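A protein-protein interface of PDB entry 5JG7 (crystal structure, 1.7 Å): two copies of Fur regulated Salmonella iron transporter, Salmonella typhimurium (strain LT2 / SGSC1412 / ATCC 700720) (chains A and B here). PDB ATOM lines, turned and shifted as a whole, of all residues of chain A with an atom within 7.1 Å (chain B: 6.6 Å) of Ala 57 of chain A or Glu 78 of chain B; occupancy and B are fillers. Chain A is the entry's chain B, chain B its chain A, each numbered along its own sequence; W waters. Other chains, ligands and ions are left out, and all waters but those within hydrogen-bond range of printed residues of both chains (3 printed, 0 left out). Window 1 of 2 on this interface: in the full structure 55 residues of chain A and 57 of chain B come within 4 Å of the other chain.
Water W2 lies within hydrogen-bond range of OG1 of Thr 83 of chain A and O of Val 76 of chain B.
Water W1 bridges O of Glu 78 of chain B (2.6 Å) and N of Val 80 of chain A (2.9 Å).
Water W3 bridges the backbone carbonyl oxygen of Glu 78 of chain A and the backbone NH of Val 80 of chain B.
Asn 58 of chain A touches Ser 82 of chain B, and with the chains exchanged Ser 82 of chain A touches Asn 58 of chain B.
Gly 59 of chain A touches Val 80 of chain B, and with the chains exchanged Val 80 of chain A touches Gly 59 of chain B.
Gly 59 of chain A touches Ser 82 of chain B, and with the chains exchanged Ser 82 of chain A touches Gly 59 of chain B.
Glu 78 of chain A touches Val 80 of chain B, and with the chains exchanged Val 80 of chain A touches Glu 78 of chain B.
Of the 32 pairs that touch across the chains among the printed residues, 8 have their exchanged pair printed and touching as well.
Printed residues of chain B that touch a printed residue of chain A: Asn 58, Gly 59, Leu 60, Asn 61, Val 76, Pro 77, Glu 78, Val 79, Val 80, Val 81 and Ser 82.
Hydrophobic or aromatic side chains of chain A that line the printed part of chain B: Ile 12, Leu 54, Ile 55, Leu 56, Ala 57, Val 80, Tyr 113 and Tyr 124.
Among the printed residues, 32 pairs touch across the chains.
Among the printed residues, no Asp or Glu carboxylate lies within 4 Å of a Lys or Arg side-chain nitrogen of the other chain.
The backbone NH (N) of Leu 60 of chain B lies within hydrogen-bond range of the side-chain carboxylate (OE2) of Glu 78 of chain B, 2.7 Å away.
The side-chain hydroxyl (OG1) of Thr 7 of chain A is in hydrogen-bond range of the backbone carbonyl oxygen (O) of Leu 56 of chain A (2.8 Å).
OH of Tyr 113 of chain A is in hydrogen-bond range of OD1 of Asn 58 of chain A (2.7 Å).
The backbone NH (N) of Ile 6 of chain A sits at hydrogen-bond distance from the backbone carbonyl oxygen (O) of Leu 54 of chain A (2.9 Å).
O of Ile 6 of chain A lies within hydrogen-bond range of N of Leu 56 of chain A, 2.9 Å away.
Of the printed residues of chain B, Ile 12 of chain A touches Val 81.
Lys 31 of chain A touches none of the printed residues of chain B.
Printed residues of chain B within 4 Å of Ala 57 of chain A: Glu 78, Val 79, Val 80, Val 81 and Ser 82.
Printed residues of chain B within 4 Å of Asn 58 of chain A: Ser 82 (3.5 Å).
Val 79 of chain A touches none of the printed residues of chain B.
Of the printed residues of chain A, Leu 60 of chain B touches Thr 8 (3.9 Å).
Printed residues of chain A within 4 Å of Val 81 of chain B: Ile 12, Leu 56, Ala 57 and Tyr 113.
The nearest residue of chain A that does not touch Glu 78 of chain B is Thr 83 of chain A (4.5 Å).
The side-chain hydroxyl of Ser 82 of chain B is in hydrogen-bond range of the backbone NH of Gly 59 of chain A, 2.8 Å away.
The backbone carbonyl oxygen (O) of Val 79 of chain B is in hydrogen-bond range of the backbone NH (N) of Ala 57 of chain A (2.9 Å).
The backbone carbonyl oxygen (O) of Ile 55 of chain A sits at hydrogen-bond distance from the backbone NH (N) of Val 79 of chain B (2.9 Å).
O of Pro 77 of chain B sits at hydrogen-bond distance from N of Ile 55 of chain A (2.9 Å).
N of Val 81 of chain B sits at hydrogen-bond distance from O of Ala 57 of chain A (2.8 Å).
OD1 of Asn 61 of chain B is in hydrogen-bond range of OG of Ser 82 of chain A, at 2.7 Å.
OG of Ser 82 of chain A is in hydrogen-bond range of N of Gly 59 of chain B (2.8 Å).
Among the printed residues, merely in contact across the chains: Thr 8 of chain A with Leu 60 of chain B (3.9 Å), Ile 12 of chain A with Val 81 of chain B (3.8 Å), Gln 53 of chain A with Val 76 of chain B (3.6 Å), Gln 53 of chain A with Pro 77 of chain B (3.4 Å), Leu 54 of chain A with Val 76 of chain B (3.5 Å), Leu 54 of chain A with Pro 77 of chain B (3.5 Å), Leu 54 of chain A with Val 79 of chain B (3.7 Å), Ile 55 of chain A with Val 76 of chain B (3.9 Å), Ile 55 of chain A with Glu 78 of chain B (3.3 Å), Leu 56 of chain A with Val 79 of chain B (3.6 Å), Leu 56 of chain A with Val 81 of chain B (3.99 Å), Ala 57 of chain A with Glu 78 of chain B (3.3 Å), Ala 57 of chain A with Val 80 of chain B (3.3 Å), Ala 57 of chain A with Ser 82 of chain B (3.999 Å), Asn 58 of chain A with Ser 82 of chain B (3.5 Å), Gly 59 of chain A with Val 80 of chain B (3.6 Å), Glu 78 of chain A with Val 80 of chain B (3.7 Å), Val 80 of chain A with Gly 59 of chain B (3.6 Å), Val 80 of chain A with Glu 78 of chain B (3.7 Å), Ser 82 of chain A with Asn 58 of chain B (3.5 Å), Thr 83 of chain A with Val 76 of chain B (3.8 Å), Tyr 113 of chain A with Val 81 of chain B (3.4 Å), Tyr 113 of chain A with Ser 82 of chain B (3.9 Å), Tyr 124 of chain A with Pro 77 of chain B (3.7 Å) and Tyr 124 of chain A with Val 79 of chain B (3.5 Å).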
ATOM      1  N   ILE A   6       2.242   5.128  10.474  1.00  0.00           N
ATOM      2  CA  ILE A   6       2.194   4.322   9.263  1.00  0.00           C
ATOM      3  C   ILE A   6       2.648   2.898   9.558  1.00  0.00           C
ATOM      4  O   ILE A   6       3.251   2.603  10.592  1.00  0.00           O
ATOM      5  CB  ILE A   6       3.025   4.915   8.100  1.00  0.00           C
ATOM      6  CG1 ILE A   6       4.529   4.920   8.417  1.00  0.00           C
ATOM      7  CG2 ILE A   6       2.517   6.328   7.763  1.00  0.00           C
ATOM      8  CD1 ILE A   6       5.424   5.237   7.206  1.00  0.00           C
ATOM      9  N   THR A   7       2.337   2.018   8.616  1.00  0.00           N
ATOM     10  CA  THR A   7       2.728   0.616   8.689  1.00  0.00           C
ATOM     11  C   THR A   7       2.719   0.060   7.279  1.00  0.00           C
ATOM     12  O   THR A   7       2.000   0.559   6.407  1.00  0.00           O
ATOM     13  CB  THR A   7       1.779  -0.182   9.604  1.00  0.00           C
ATOM     14  OG1 THR A   7       2.240  -1.531   9.739  1.00  0.00           O
ATOM     15  CG2 THR A   7       0.344  -0.174   9.066  1.00  0.00           C
ATOM     16  N   THR A   8       3.529  -0.966   7.053  1.00  0.00           N
ATOM     17  CA  THR A   8       3.436  -1.686   5.785  1.00  0.00           C
ATOM     18  C   THR A   8       2.501  -2.883   5.860  1.00  0.00           C
ATOM     19  O   THR A   8       2.282  -3.544   4.839  1.00  0.00           O
ATOM     20  CB  THR A   8       4.819  -2.159   5.314  1.00  0.00           C
ATOM     21  OG1 THR A   8       5.335  -3.161   6.202  1.00  0.00           O
ATOM     22  CG2 THR A   8       5.800  -0.984   5.206  1.00  0.00           C
ATOM     23  N   PHE A   9       1.953  -3.178   7.034  1.00  0.00           N
ATOM     24  CA  PHE A   9       1.135  -4.361   7.255  1.00  0.00           C
ATOM     25  C   PHE A   9      -0.312  -3.924   7.378  1.00  0.00           C
ATOM     26  O   PHE A   9      -0.672  -3.221   8.327  1.00  0.00           O
ATOM     27  CB  PHE A   9       1.580  -5.108   8.509  1.00  0.00           C
ATOM     28  CG  PHE A   9       3.014  -5.531   8.470  1.00  0.00           C
ATOM     29  CD1 PHE A   9       3.377  -6.728   7.872  1.00  0.00           C
ATOM     30  CD2 PHE A   9       4.005  -4.724   9.013  1.00  0.00           C
ATOM     31  CE1 PHE A   9       4.707  -7.122   7.829  1.00  0.00           C
ATOM     32  CE2 PHE A   9       5.337  -5.107   8.975  1.00  0.00           C
ATOM     33  CZ  PHE A   9       5.683  -6.315   8.373  1.00  0.00           C
ATOM     34  N   ILE A  12      -2.267  -4.542  10.653  1.00  0.00           N
ATOM     35  CA  ILE A  12      -1.867  -3.648  11.739  1.00  0.00           C
ATOM     36  C   ILE A  12      -2.551  -2.305  11.573  1.00  0.00           C
ATOM     37  O   ILE A  12      -3.025  -1.713  12.549  1.00  0.00           O
ATOM     38  CB  ILE A  12      -0.331  -3.498  11.812  1.00  0.00           C
ATOM     39  CG1 ILE A  12       0.299  -4.774  12.359  1.00  0.00           C
ATOM     40  CG2 ILE A  12       0.068  -2.309  12.717  1.00  0.00           C
ATOM     41  CD1 ILE A  12       1.815  -4.754  12.335  1.00  0.00           C
ATOM     42  N   LYS A  31       4.704  -2.260   0.615  1.00  0.00           N
ATOM     43  CA  LYS A  31       6.066  -2.764   0.570  1.00  0.00           C
ATOM     44  C   LYS A  31       6.245  -3.587  -0.698  1.00  0.00           C
ATOM     45  O   LYS A  31       5.505  -4.559  -0.898  1.00  0.00           O
ATOM     46  CB  LYS A  31       6.345  -3.614   1.801  1.00  0.00           C
ATOM     47  CG  LYS A  31       7.708  -4.287   1.838  1.00  0.00           C
ATOM     48  CD  LYS A  31       7.953  -4.921   3.208  1.00  0.00           C
ATOM     49  CE  LYS A  31       9.216  -4.369   3.858  1.00  0.00           C
ATOM     50  NZ  LYS A  31       9.387  -4.844   5.257  1.00  0.00           N
ATOM     51  N   GLN A  53       5.048  10.033  12.182  1.00  0.00           N
ATOM     52  CA  GLN A  53       5.781  10.182  13.428  1.00  0.00           C
ATOM     53  C   GLN A  53       6.050   8.859  14.118  1.00  0.00           C
ATOM     54  O   GLN A  53       6.753   8.837  15.135  1.00  0.00           O
ATOM     55  CB  GLN A  53       5.007  11.102  14.381  1.00  0.00           C
ATOM     56  CG  GLN A  53       4.761  12.478  13.806  1.00  0.00           C
ATOM     57  CD  GLN A  53       3.712  13.238  14.583  1.00  0.00           C
ATOM     58  OE1 GLN A  53       2.519  13.141  14.293  1.00  0.00           O
ATOM     59  NE2 GLN A  53       4.148  13.984  15.593  1.00  0.00           N
ATOM     60  N   LEU A  54       5.509   7.765  13.596  1.00  0.00           N
ATOM     61  CA  LEU A  54       5.679   6.451  14.190  1.00  0.00           C
ATOM     62  C   LEU A  54       5.394   5.422  13.112  1.00  0.00           C
ATOM     63  O   LEU A  54       4.460   5.591  12.328  1.00  0.00           O
ATOM     64  CB  LEU A  54       4.739   6.252  15.384  1.00  0.00           C
ATOM     65  CG  LEU A  54       4.756   4.904  16.106  1.00  0.00           C
ATOM     66  CD1 LEU A  54       6.109   4.629  16.760  1.00  0.00           C
ATOM     67  CD2 LEU A  54       3.629   4.843  17.136  1.00  0.00           C
ATOM     68  N   ILE A  55       6.214   4.380  13.077  1.00  0.00           N
ATOM     69  CA  ILE A  55       6.020   3.224  12.208  1.00  0.00           C
ATOM     70  C   ILE A  55       5.720   2.037  13.108  1.00  0.00           C
ATOM     71  O   ILE A  55       6.446   1.796  14.081  1.00  0.00           O
ATOM     72  CB  ILE A  55       7.276   2.947  11.358  1.00  0.00           C
ATOM     73  CG1 ILE A  55       7.619   4.137  10.449  1.00  0.00           C
ATOM     74  CG2 ILE A  55       7.108   1.626  10.573  1.00  0.00           C
ATOM     75  CD1 ILE A  55       9.102   4.152  10.009  1.00  0.00           C
ATOM     76  N   LEU A  56       4.654   1.303  12.799  1.00  0.00           N
ATOM     77  CA  LEU A  56       4.319   0.079  13.517  1.00  0.00           C
ATOM     78  C   LEU A  56       4.705  -1.111  12.654  1.00  0.00           C
ATOM     79  O   LEU A  56       4.387  -1.142  11.459  1.00  0.00           O
ATOM     80  CB  LEU A  56       2.827   0.019  13.844  1.00  0.00           C
ATOM     81  CG  LEU A  56       2.309   1.213  14.629  1.00  0.00           C
ATOM     82  CD1 LEU A  56       0.808   1.008  14.893  1.00  0.00           C
ATOM     83  CD2 LEU A  56       3.075   1.370  15.936  1.00  0.00           C
ATOM     84  N   ALA A  57       5.369  -2.092  13.258  1.00  0.00           N
ATOM     85  CA  ALA A  57       5.980  -3.170  12.490  1.00  0.00           C
ATOM     86  C   ALA A  57       5.735  -4.527  13.132  1.00  0.00           C
ATOM     87  O   ALA A  57       5.571  -4.638  14.346  1.00  0.00           O
ATOM     88  CB  ALA A  57       7.485  -2.958  12.372  1.00  0.00           C
ATOM     89  N   ASN A  58       5.730  -5.562  12.293  1.00  0.00           N
ATOM     90  CA  ASN A  58       5.917  -6.924  12.764  1.00  0.00           C
ATOM     91  C   ASN A  58       7.392  -7.178  13.032  1.00  0.00           C
ATOM     92  O   ASN A  58       8.274  -6.595  12.391  1.00  0.00           O
ATOM     93  CB  ASN A  58       5.421  -7.937  11.734  1.00  0.00           C
ATOM     94  CG  ASN A  58       3.928  -8.117  11.766  1.00  0.00           C
ATOM     95  OD1 ASN A  58       3.292  -7.964  12.806  1.00  0.00           O
ATOM     96  ND2 ASN A  58       3.357  -8.459  10.620  1.00  0.00           N
ATOM     97  N   GLY A  59       7.660  -8.063  13.988  1.00  0.00           N
ATOM     98  CA  GLY A  59       9.013  -8.417  14.348  1.00  0.00           C
ATOM     99  C   GLY A  59       9.437  -9.765  13.799  1.00  0.00           C
ATOM    100  O   GLY A  59       8.747 -10.406  12.998  1.00  0.00           O
ATOM    101  N   GLU A  78      11.804  -6.768  20.926  1.00  0.00           N
ATOM    102  CA  GLU A  78      12.650  -6.508  19.767  1.00  0.00           C
ATOM    103  C   GLU A  78      12.659  -5.011  19.523  1.00  0.00           C
ATOM    104  O   GLU A  78      11.595  -4.399  19.401  1.00  0.00           O
ATOM    105  CB  GLU A  78      12.153  -7.251  18.525  1.00  0.00           C
ATOM    106  CG  GLU A  78      12.946  -6.922  17.241  1.00  0.00           C
ATOM    107  CD  GLU A  78      12.588  -7.831  16.069  1.00  0.00           C
ATOM    108  OE1 GLU A  78      13.266  -7.764  15.011  1.00  0.00           O
ATOM    109  OE2 GLU A  78      11.626  -8.620  16.196  1.00  0.00           O
ATOM    110  N   VAL A  79      13.853  -4.420  19.459  1.00  0.00           N
ATOM    111  CA  VAL A  79      14.012  -2.976  19.405  1.00  0.00           C
ATOM    112  C   VAL A  79      14.742  -2.631  18.119  1.00  0.00           C
ATOM    113  O   VAL A  79      15.803  -3.200  17.836  1.00  0.00           O
ATOM    114  CB  VAL A  79      14.782  -2.442  20.630  1.00  0.00           C
ATOM    115  CG1 VAL A  79      15.172  -0.985  20.410  1.00  0.00           C
ATOM    116  CG2 VAL A  79      13.931  -2.588  21.894  1.00  0.00           C
ATOM    117  N   VAL A  80      14.169  -1.716  17.340  1.00  0.00           N
ATOM    118  CA  VAL A  80      14.822  -1.190  16.140  1.00  0.00           C
ATOM    119  C   VAL A  80      15.905  -0.207  16.576  1.00  0.00           C
ATOM    120  O   VAL A  80      15.601   0.810  17.206  1.00  0.00           O
ATOM    121  CB  VAL A  80      13.799  -0.508  15.222  1.00  0.00           C
ATOM    122  CG1 VAL A  80      14.523   0.266  14.086  1.00  0.00           C
ATOM    123  CG2 VAL A  80      12.843  -1.555  14.635  1.00  0.00           C
ATOM    124  N   VAL A  81      17.168  -0.503  16.235  1.00  0.00           N
ATOM    125  CA  VAL A  81      18.297   0.336  16.651  1.00  0.00           C
ATOM    126  C   VAL A  81      18.899   1.115  15.486  1.00  0.00           C
ATOM    127  O   VAL A  81      19.929   1.786  15.662  1.00  0.00           O
ATOM    128  CB  VAL A  81      19.392  -0.474  17.383  1.00  0.00           C
ATOM    129  CG1 VAL A  81      18.868  -1.038  18.717  1.00  0.00           C
ATOM    130  CG2 VAL A  81      19.956  -1.597  16.491  1.00  0.00           C
ATOM    131  N   SER A  82      18.276   1.076  14.308  1.00  0.00           N
ATOM    132  CA  SER A  82      18.787   1.810  13.148  1.00  0.00           C
ATOM    133  C   SER A  82      18.173   3.201  12.978  1.00  0.00           C
ATOM    134  O   SER A  82      18.461   3.874  11.980  1.00  0.00           O
ATOM    135  CB  SER A  82      18.557   0.999  11.872  1.00  0.00           C
ATOM    136  OG  SER A  82      17.167   0.802  11.654  1.00  0.00           O
ATOM    137  N   THR A  83      17.322   3.642  13.897  1.00  0.00           N
ATOM    138  CA  THR A  83      16.640   4.927  13.747  1.00  0.00           C
ATOM    139  C   THR A  83      17.649   6.064  13.629  1.00  0.00           C
ATOM    140  O   THR A  83      18.528   6.211  14.483  1.00  0.00           O
ATOM    141  CB  THR A  83      15.720   5.154  14.937  1.00  0.00           C
ATOM    142  OG1 THR A  83      14.878   3.996  15.098  1.00  0.00           O
ATOM    143  CG2 THR A  83      14.853   6.390  14.720  1.00  0.00           C
ATOM    144  N   TYR A 113      -1.784  -8.015  19.880  1.00  0.00           N
ATOM    145  CA  TYR A 113      -1.505  -6.898  18.974  1.00  0.00           C
ATOM    146  C   TYR A 113      -2.106  -5.596  19.487  1.00  0.00           C
ATOM    147  O   TYR A 113      -1.469  -4.540  19.448  1.00  0.00           O
ATOM    148  CB  TYR A 113      -2.067  -7.180  17.581  1.00  0.00           C
ATOM    149  CG  TYR A 113      -1.149  -7.794  16.558  1.00  0.00           C
ATOM    150  CD1 TYR A 113      -0.033  -7.105  16.073  1.00  0.00           C
ATOM    151  CD2 TYR A 113      -1.446  -9.039  16.012  1.00  0.00           C
ATOM    152  CE1 TYR A 113       0.767  -7.651  15.092  1.00  0.00           C
ATOM    153  CE2 TYR A 113      -0.647  -9.597  15.039  1.00  0.00           C
ATOM    154  CZ  TYR A 113       0.455  -8.900  14.581  1.00  0.00           C
ATOM    155  OH  TYR A 113       1.242  -9.444  13.604  1.00  0.00           O
ATOM    156  N   TYR A 124       4.335   7.233  22.427  1.00  0.00           N
ATOM    157  CA  TYR A 124       4.799   8.226  21.469  1.00  0.00           C
ATOM    158  C   TYR A 124       3.840   9.387  21.305  1.00  0.00           C
ATOM    159  O   TYR A 124       4.244  10.440  20.796  1.00  0.00           O
ATOM    160  CB  TYR A 124       5.075   7.555  20.107  1.00  0.00           C
ATOM    161  CG  TYR A 124       6.379   6.818  20.153  1.00  0.00           C
ATOM    162  CD1 TYR A 124       7.584   7.495  19.977  1.00  0.00           C
ATOM    163  CD2 TYR A 124       6.423   5.473  20.478  1.00  0.00           C
ATOM    164  CE1 TYR A 124       8.791   6.835  20.063  1.00  0.00           C
ATOM    165  CE2 TYR A 124       7.628   4.801  20.565  1.00  0.00           C
ATOM    166  CZ  TYR A 124       8.804   5.490  20.363  1.00  0.00           C
ATOM    167  OH  TYR A 124       9.994   4.822  20.460  1.00  0.00           O
ATOM    168  N   ASN B  58      17.458  -4.089  12.692  1.00  0.00           N
ATOM    169  CA  ASN B  58      17.395  -2.984  11.748  1.00  0.00           C
ATOM    170  C   ASN B  58      15.944  -2.712  11.389  1.00  0.00           C
ATOM    171  O   ASN B  58      15.087  -3.603  11.450  1.00  0.00           O
ATOM    172  CB  ASN B  58      18.180  -3.305  10.478  1.00  0.00           C
ATOM    173  CG  ASN B  58      19.659  -3.044  10.625  1.00  0.00           C
ATOM    174  OD1 ASN B  58      20.072  -2.146  11.356  1.00  0.00           O
ATOM    175  ND2 ASN B  58      20.470  -3.805   9.898  1.00  0.00           N
ATOM    176  N   GLY B  59      15.661  -1.458  11.036  1.00  0.00           N
ATOM    177  CA  GLY B  59      14.313  -1.034  10.745  1.00  0.00           C
ATOM    178  C   GLY B  59      14.043  -0.886   9.256  1.00  0.00           C
ATOM    179  O   GLY B  59      14.871  -1.168   8.388  1.00  0.00           O
ATOM    180  N   LEU B  60      12.819  -0.441   8.978  1.00  0.00           N
ATOM    181  CA  LEU B  60      12.398  -0.197   7.610  1.00  0.00           C
ATOM    182  C   LEU B  60      13.314   0.806   6.914  1.00  0.00           C
ATOM    183  O   LEU B  60      13.519   0.729   5.695  1.00  0.00           O
ATOM    184  CB  LEU B  60      10.949   0.290   7.657  1.00  0.00           C
ATOM    185  CG  LEU B  60      10.163   0.530   6.389  1.00  0.00           C
ATOM    186  CD1 LEU B  60      10.140  -0.741   5.576  1.00  0.00           C
ATOM    187  CD2 LEU B  60       8.763   0.953   6.818  1.00  0.00           C
ATOM    188  N   ASN B  61      13.902   1.732   7.676  1.00  0.00           N
ATOM    189  CA  ASN B  61      14.751   2.757   7.093  1.00  0.00           C
ATOM    190  C   ASN B  61      16.019   2.193   6.466  1.00  0.00           C
ATOM    191  O   ASN B  61      16.721   2.934   5.773  1.00  0.00           O
ATOM    192  CB  ASN B  61      15.091   3.837   8.141  1.00  0.00           C
ATOM    193  CG  ASN B  61      16.045   3.350   9.241  1.00  0.00           C
ATOM    194  OD1 ASN B  61      16.055   2.178   9.626  1.00  0.00           O
ATOM    195  ND2 ASN B  61      16.834   4.276   9.770  1.00  0.00           N
ATOM    196  N   VAL B  76      12.353   8.521  11.906  1.00  0.00           N
ATOM    197  CA  VAL B  76      11.040   8.238  12.481  1.00  0.00           C
ATOM    198  C   VAL B  76      11.137   6.958  13.311  1.00  0.00           C
ATOM    199  O   VAL B  76      11.627   5.936  12.796  1.00  0.00           O
ATOM    200  CB  VAL B  76       9.996   8.093  11.388  1.00  0.00           C
ATOM    201  CG1 VAL B  76       8.664   7.615  11.982  1.00  0.00           C
ATOM    202  CG2 VAL B  76       9.832   9.408  10.641  1.00  0.00           C
ATOM    203  N   PRO B  77      10.685   6.976  14.559  1.00  0.00           N
ATOM    204  CA  PRO B  77      10.760   5.762  15.378  1.00  0.00           C
ATOM    205  C   PRO B  77       9.897   4.649  14.807  1.00  0.00           C
ATOM    206  O   PRO B  77       8.838   4.887  14.220  1.00  0.00           O
ATOM    207  CB  PRO B  77      10.246   6.213  16.750  1.00  0.00           C
ATOM    208  CG  PRO B  77       9.588   7.547  16.534  1.00  0.00           C
ATOM    209  CD  PRO B  77      10.181   8.145  15.298  1.00  0.00           C
ATOM    210  N   GLU B  78      10.378   3.423  14.985  1.00  0.00           N
ATOM    211  CA  GLU B  78       9.686   2.224  14.528  1.00  0.00           C
ATOM    212  C   GLU B  78       9.575   1.247  15.691  1.00  0.00           C
ATOM    213  O   GLU B  78      10.583   0.932  16.328  1.00  0.00           O
ATOM    214  CB  GLU B  78      10.437   1.584  13.356  1.00  0.00           C
ATOM    215  CG  GLU B  78       9.786   0.308  12.849  1.00  0.00           C
ATOM    216  CD  GLU B  78      10.444  -0.224  11.589  1.00  0.00           C
ATOM    217  OE1 GLU B  78       9.974  -1.263  11.083  1.00  0.00           O
ATOM    218  OE2 GLU B  78      11.418   0.394  11.096  1.00  0.00           O
ATOM    219  N   VAL B  79       8.361   0.751  15.957  1.00  0.00           N
ATOM    220  CA  VAL B  79       8.083  -0.085  17.120  1.00  0.00           C
ATOM    221  C   VAL B  79       7.520  -1.417  16.639  1.00  0.00           C
ATOM    222  O   VAL B  79       6.582  -1.444  15.830  1.00  0.00           O
ATOM    223  CB  VAL B  79       7.100   0.593  18.096  1.00  0.00           C
ATOM    224  CG1 VAL B  79       6.697  -0.392  19.197  1.00  0.00           C
ATOM    225  CG2 VAL B  79       7.715   1.855  18.704  1.00  0.00           C
ATOM    226  N   VAL B  80       8.090  -2.514  17.135  1.00  0.00           N
ATOM    227  CA  VAL B  80       7.579  -3.859  16.871  1.00  0.00           C
ATOM    228  C   VAL B  80       6.368  -4.086  17.768  1.00  0.00           C
ATOM    229  O   VAL B  80       6.475  -3.961  18.994  1.00  0.00           O
ATOM    230  CB  VAL B  80       8.663  -4.914  17.123  1.00  0.00           C
ATOM    231  CG1 VAL B  80       8.069  -6.327  17.103  1.00  0.00           C
ATOM    232  CG2 VAL B  80       9.754  -4.777  16.065  1.00  0.00           C
ATOM    233  N   VAL B  81       5.221  -4.412  17.164  1.00  0.00           N
ATOM    234  CA  VAL B  81       3.968  -4.608  17.904  1.00  0.00           C
ATOM    235  C   VAL B  81       3.484  -6.053  17.862  1.00  0.00           C
ATOM    236  O   VAL B  81       2.373  -6.343  18.332  1.00  0.00           O
ATOM    237  CB  VAL B  81       2.858  -3.659  17.409  1.00  0.00           C
ATOM    238  CG1 VAL B  81       3.180  -2.202  17.716  1.00  0.00           C
ATOM    239  CG2 VAL B  81       2.571  -3.863  15.905  1.00  0.00           C
ATOM    240  N   SER B  82       4.274  -6.977  17.319  1.00  0.00           N
ATOM    241  CA  SER B  82       3.895  -8.389  17.286  1.00  0.00           C
ATOM    242  C   SER B  82       4.434  -9.181  18.472  1.00  0.00           C
ATOM    243  O   SER B  82       4.307 -10.413  18.489  1.00  0.00           O
ATOM    244  CB  SER B  82       4.391  -9.038  15.992  1.00  0.00           C
ATOM    245  OG  SER B  82       5.809  -8.977  15.919  1.00  0.00           O
ATOM    246  N   THR B  83       5.072  -8.521  19.431  1.00  0.00           N
ATOM    247  CA  THR B  83       5.704  -9.224  20.537  1.00  0.00           C
ATOM    248  C   THR B  83       4.670 -10.018  21.321  1.00  0.00           C
ATOM    249  O   THR B  83       3.680  -9.456  21.782  1.00  0.00           O
ATOM    250  CB  THR B  83       6.402  -8.227  21.448  1.00  0.00           C
ATOM    251  OG1 THR B  83       7.339  -7.474  20.665  1.00  0.00           O
ATOM    252  CG2 THR B  83       7.145  -8.961  22.567  1.00  0.00           C
HETATM  253  O   HOH W   1      11.813  -0.268  18.313  1.00  0.00           O
HETATM  254  O   HOH W   2      13.356   3.691  13.104  1.00  0.00           O
HETATM  255  O   HOH W   3      10.148  -2.139  19.181  1.00  0.00           O
